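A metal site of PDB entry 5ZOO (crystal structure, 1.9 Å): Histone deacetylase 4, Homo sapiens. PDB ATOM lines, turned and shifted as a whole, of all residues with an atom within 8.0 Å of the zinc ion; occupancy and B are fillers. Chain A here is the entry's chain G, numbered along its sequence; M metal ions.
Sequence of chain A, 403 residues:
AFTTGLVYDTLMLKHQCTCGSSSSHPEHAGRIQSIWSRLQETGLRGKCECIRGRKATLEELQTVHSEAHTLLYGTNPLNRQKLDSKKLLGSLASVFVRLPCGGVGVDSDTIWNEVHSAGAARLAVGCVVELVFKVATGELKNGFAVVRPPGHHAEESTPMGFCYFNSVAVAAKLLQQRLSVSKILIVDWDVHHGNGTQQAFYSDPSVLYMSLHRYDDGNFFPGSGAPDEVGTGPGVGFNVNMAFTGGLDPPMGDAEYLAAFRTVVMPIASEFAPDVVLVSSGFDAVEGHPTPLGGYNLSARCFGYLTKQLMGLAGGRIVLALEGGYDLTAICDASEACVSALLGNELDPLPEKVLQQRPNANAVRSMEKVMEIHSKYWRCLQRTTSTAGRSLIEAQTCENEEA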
ATOM      1  N   GLN A  16      22.746 -31.843 -20.927  1.00  0.00           N
ATOM      2  CA  GLN A  16      23.026 -30.468 -21.339  1.00  0.00           C
ATOM      3  C   GLN A  16      24.403 -30.068 -20.855  1.00  0.00           C
ATOM      4  O   GLN A  16      24.800 -30.416 -19.737  1.00  0.00           O
ATOM      5  CB  GLN A  16      21.951 -29.519 -20.789  1.00  0.00           C
ATOM      6  CG  GLN A  16      22.206 -28.059 -21.091  1.00  0.00           C
ATOM      7  CD  GLN A  16      20.961 -27.216 -20.898  1.00  0.00           C
ATOM      8  OE1 GLN A  16      19.869 -27.742 -20.683  1.00  0.00           O
ATOM      9  NE2 GLN A  16      21.119 -25.897 -20.986  1.00  0.00           N
ATOM     10  N   CYS A  17      25.129 -29.327 -21.691  1.00  0.00           N
ATOM     11  CA  CYS A  17      26.439 -28.846 -21.281  1.00  0.00           C
ATOM     12  C   CYS A  17      26.294 -27.818 -20.159  1.00  0.00           C
ATOM     13  O   CYS A  17      25.282 -27.117 -20.049  1.00  0.00           O
ATOM     14  CB  CYS A  17      27.194 -28.228 -22.457  1.00  0.00           C
ATOM     15  SG  CYS A  17      28.958 -28.070 -22.116  1.00  0.00           S
ATOM     16  N   THR A  18      27.315 -27.755 -19.316  1.00  0.00           N
ATOM     17  CA  THR A  18      27.319 -26.834 -18.181  1.00  0.00           C
ATOM     18  C   THR A  18      27.886 -25.475 -18.524  1.00  0.00           C
ATOM     19  O   THR A  18      27.951 -24.608 -17.651  1.00  0.00           O
ATOM     20  CB  THR A  18      28.130 -27.448 -17.040  1.00  0.00           C
ATOM     21  OG1 THR A  18      29.452 -27.718 -17.518  1.00  0.00           O
ATOM     22  CG2 THR A  18      27.480 -28.744 -16.577  1.00  0.00           C
ATOM     23  N   CYS A  19      28.285 -25.249 -19.780  1.00  0.00           N
ATOM     24  CA  CYS A  19      29.113 -24.086 -20.111  1.00  0.00           C
ATOM     25  C   CYS A  19      28.323 -22.783 -20.143  1.00  0.00           C
ATOM     26  O   CYS A  19      28.907 -21.721 -19.920  1.00  0.00           O
ATOM     27  CB  CYS A  19      29.820 -24.297 -21.448  1.00  0.00           C
ATOM     28  SG  CYS A  19      28.705 -24.460 -22.880  1.00  0.00           S
ATOM     29  N   GLY A  20      27.029 -22.839 -20.420  1.00  0.00           N
ATOM     30  CA  GLY A  20      26.258 -21.615 -20.561  1.00  0.00           C
ATOM     31  C   GLY A  20      26.455 -20.870 -21.857  1.00  0.00           C
ATOM     32  O   GLY A  20      26.133 -19.682 -21.938  1.00  0.00           O
ATOM     33  N   SER A  21      26.997 -21.525 -22.887  1.00  0.00           N
ATOM     34  CA  SER A  21      27.252 -20.917 -24.188  1.00  0.00           C
ATOM     35  C   SER A  21      26.241 -21.513 -25.176  1.00  0.00           C
ATOM     36  O   SER A  21      26.533 -22.482 -25.870  1.00  0.00           O
ATOM     37  CB  SER A  21      28.695 -21.157 -24.639  1.00  0.00           C
ATOM     38  OG  SER A  21      28.975 -20.517 -25.881  1.00  0.00           O
ATOM     39  N   SER A  22      25.048 -20.901 -25.230  1.00  0.00           N
ATOM     40  CA  SER A  22      23.916 -21.508 -25.932  1.00  0.00           C
ATOM     41  C   SER A  22      24.202 -21.724 -27.409  1.00  0.00           C
ATOM     42  O   SER A  22      23.795 -22.734 -27.991  1.00  0.00           O
ATOM     43  CB  SER A  22      22.665 -20.655 -25.750  1.00  0.00           C
ATOM     44  OG  SER A  22      22.289 -20.587 -24.391  1.00  0.00           O
ATOM     45  N   SER A  24      26.732 -22.619 -28.886  1.00  0.00           N
ATOM     46  CA  SER A  24      27.809 -23.552 -29.168  1.00  0.00           C
ATOM     47  C   SER A  24      27.357 -24.992 -29.354  1.00  0.00           C
ATOM     48  O   SER A  24      28.136 -25.797 -29.886  1.00  0.00           O
ATOM     49  CB  SER A  24      28.857 -23.509 -28.045  1.00  0.00           C
ATOM     50  OG  SER A  24      29.422 -22.218 -27.932  1.00  0.00           O
ATOM     51  N   HIS A  25      26.144 -25.343 -28.947  1.00  0.00           N
ATOM     52  CA  HIS A  25      25.719 -26.737 -28.919  1.00  0.00           C
ATOM     53  C   HIS A  25      24.397 -26.895 -29.654  1.00  0.00           C
ATOM     54  O   HIS A  25      23.314 -26.677 -29.062  1.00  0.00           O
ATOM     55  CB  HIS A  25      25.608 -27.233 -27.479  1.00  0.00           C
ATOM     56  CG  HIS A  25      26.888 -27.120 -26.711  1.00  0.00           C
ATOM     57  ND1 HIS A  25      28.048 -27.740 -27.120  1.00  0.00           N
ATOM     58  CD2 HIS A  25      27.182 -26.471 -25.565  1.00  0.00           C
ATOM     59  CE1 HIS A  25      29.019 -27.470 -26.262  1.00  0.00           C
ATOM     60  NE2 HIS A  25      28.516 -26.699 -25.308  1.00  0.00           N
ATOM     61  N   LEU A  99      36.422 -29.205 -22.663  1.00  0.00           N
ATOM     62  CA  LEU A  99      36.155 -28.604 -23.954  1.00  0.00           C
ATOM     63  C   LEU A  99      36.475 -27.113 -23.919  1.00  0.00           C
ATOM     64  O   LEU A  99      36.468 -26.478 -22.861  1.00  0.00           O
ATOM     65  CB  LEU A  99      34.693 -28.797 -24.329  1.00  0.00           C
ATOM     66  CG  LEU A  99      34.172 -30.228 -24.510  1.00  0.00           C
ATOM     67  CD1 LEU A  99      32.709 -30.187 -24.924  1.00  0.00           C
ATOM     68  CD2 LEU A  99      34.988 -30.976 -25.544  1.00  0.00           C
ATOM     69  N   PRO A 100      36.760 -26.515 -25.093  1.00  0.00           N
ATOM     70  CA  PRO A 100      36.997 -25.064 -25.123  1.00  0.00           C
ATOM     71  C   PRO A 100      35.822 -24.246 -24.610  1.00  0.00           C
ATOM     72  O   PRO A 100      36.022 -23.125 -24.141  1.00  0.00           O
ATOM     73  CB  PRO A 100      37.271 -24.790 -26.612  1.00  0.00           C
ATOM     74  CG  PRO A 100      37.776 -26.085 -27.138  1.00  0.00           C
ATOM     75  CD  PRO A 100      37.001 -27.138 -26.399  1.00  0.00           C
ATOM     76  N   CYS A 101      34.594 -24.774 -24.677  1.00  0.00           N
ATOM     77  CA  CYS A 101      33.466 -24.039 -24.114  1.00  0.00           C
ATOM     78  C   CYS A 101      33.529 -23.980 -22.596  1.00  0.00           C
ATOM     79  O   CYS A 101      32.835 -23.150 -21.997  1.00  0.00           O
ATOM     80  CB  CYS A 101      32.139 -24.667 -24.538  1.00  0.00           C
ATOM     81  SG  CYS A 101      31.858 -26.339 -23.905  1.00  0.00           S
ATOM     82  N   GLY A 102      34.352 -24.810 -21.964  1.00  0.00           N
ATOM     83  CA  GLY A 102      34.412 -24.899 -20.512  1.00  0.00           C
ATOM     84  C   GLY A 102      33.735 -26.142 -19.951  1.00  0.00           C
ATOM     85  O   GLY A 102      33.982 -26.479 -18.780  1.00  0.00           O
ATOM     86  N   GLY A 103      32.916 -26.823 -20.736  1.00  0.00           N
ATOM     87  CA  GLY A 103      32.303 -28.052 -20.299  1.00  0.00           C
ATOM     88  C   GLY A 103      33.199 -29.258 -20.517  1.00  0.00           C
ATOM     89  O   GLY A 103      34.399 -29.151 -20.785  1.00  0.00           O
ATOM     90  N   VAL A 104      32.593 -30.436 -20.385  1.00  0.00           N
ATOM     91  CA  VAL A 104      33.260 -31.710 -20.569  1.00  0.00           C
ATOM     92  C   VAL A 104      32.583 -32.427 -21.738  1.00  0.00           C
ATOM     93  O   VAL A 104      31.378 -32.290 -21.957  1.00  0.00           O
ATOM     94  CB  VAL A 104      33.184 -32.563 -19.271  1.00  0.00           C
ATOM     95  CG1 VAL A 104      33.735 -33.957 -19.491  1.00  0.00           C
ATOM     96  CG2 VAL A 104      33.938 -31.869 -18.142  1.00  0.00           C
ATOM     97  N   GLY A 105      33.380 -33.166 -22.515  1.00  0.00           N
ATOM     98  CA  GLY A 105      32.794 -33.953 -23.589  1.00  0.00           C
ATOM     99  C   GLY A 105      33.711 -35.083 -24.012  1.00  0.00           C
ATOM    100  O   GLY A 105      34.808 -35.253 -23.483  1.00  0.00           O
ATOM    101  N   SER A 108      34.637 -32.494 -29.610  1.00  0.00           N
ATOM    102  CA  SER A 108      34.151 -31.113 -29.667  1.00  0.00           C
ATOM    103  C   SER A 108      32.645 -31.051 -29.920  1.00  0.00           C
ATOM    104  O   SER A 108      32.003 -30.073 -29.528  1.00  0.00           O
ATOM    105  CB  SER A 108      34.907 -30.339 -30.744  1.00  0.00           C
ATOM    106  OG  SER A 108      34.834 -30.973 -32.018  1.00  0.00           O
ATOM    107  N   ILE A 111      28.885 -33.471 -25.961  1.00  0.00           N
ATOM    108  CA  ILE A 111      29.106 -33.050 -24.584  1.00  0.00           C
ATOM    109  C   ILE A 111      28.789 -34.199 -23.632  1.00  0.00           C
ATOM    110  O   ILE A 111      28.100 -35.168 -23.974  1.00  0.00           O
ATOM    111  CB  ILE A 111      28.278 -31.804 -24.249  1.00  0.00           C
ATOM    112  CG1 ILE A 111      26.783 -32.129 -24.259  1.00  0.00           C
ATOM    113  CG2 ILE A 111      28.581 -30.696 -25.239  1.00  0.00           C
ATOM    114  CD1 ILE A 111      26.165 -32.319 -22.881  1.00  0.00           C
ATOM    115  N   TRP A 112      29.281 -34.083 -22.406  1.00  0.00           N
ATOM    116  CA  TRP A 112      28.997 -35.039 -21.348  1.00  0.00           C
ATOM    117  C   TRP A 112      28.668 -34.273 -20.082  1.00  0.00           C
ATOM    118  O   TRP A 112      29.502 -33.520 -19.578  1.00  0.00           O
ATOM    119  CB  TRP A 112      30.188 -35.977 -21.098  1.00  0.00           C
ATOM    120  CG  TRP A 112      29.876 -37.038 -20.086  1.00  0.00           C
ATOM    121  CD1 TRP A 112      30.340 -37.103 -18.790  1.00  0.00           C
ATOM    122  CD2 TRP A 112      29.029 -38.163 -20.261  1.00  0.00           C
ATOM    123  NE1 TRP A 112      29.827 -38.219 -18.172  1.00  0.00           N
ATOM    124  CE2 TRP A 112      29.026 -38.888 -19.049  1.00  0.00           C
ATOM    125  CE3 TRP A 112      28.280 -38.637 -21.337  1.00  0.00           C
ATOM    126  CZ2 TRP A 112      28.288 -40.058 -18.894  1.00  0.00           C
ATOM    127  CZ3 TRP A 112      27.546 -39.804 -21.173  1.00  0.00           C
ATOM    128  CH2 TRP A 112      27.565 -40.501 -19.957  1.00  0.00           C
HETATM  129 ZN    ZN M   1      29.580 -26.375 -23.607  1.00  0.00          ZN
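The backbone NH (N) of Ser 21 lies close to the side-chain sulfur (SG) of Cys 19 (3.4 Å). SG of Cys 101 lies close to N of Gly 103 (3.4 Å).
The nearest printed residue that does not touch the zinc ion is Gly 103 (4.4 Å).
The zinc ion is bound by NE2 of His 25 (2.0 Å), SG of Cys 19 (2.2 Å), SG of Cys 101 (2.3 Å) and SG of Cys 17 (2.3 Å).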
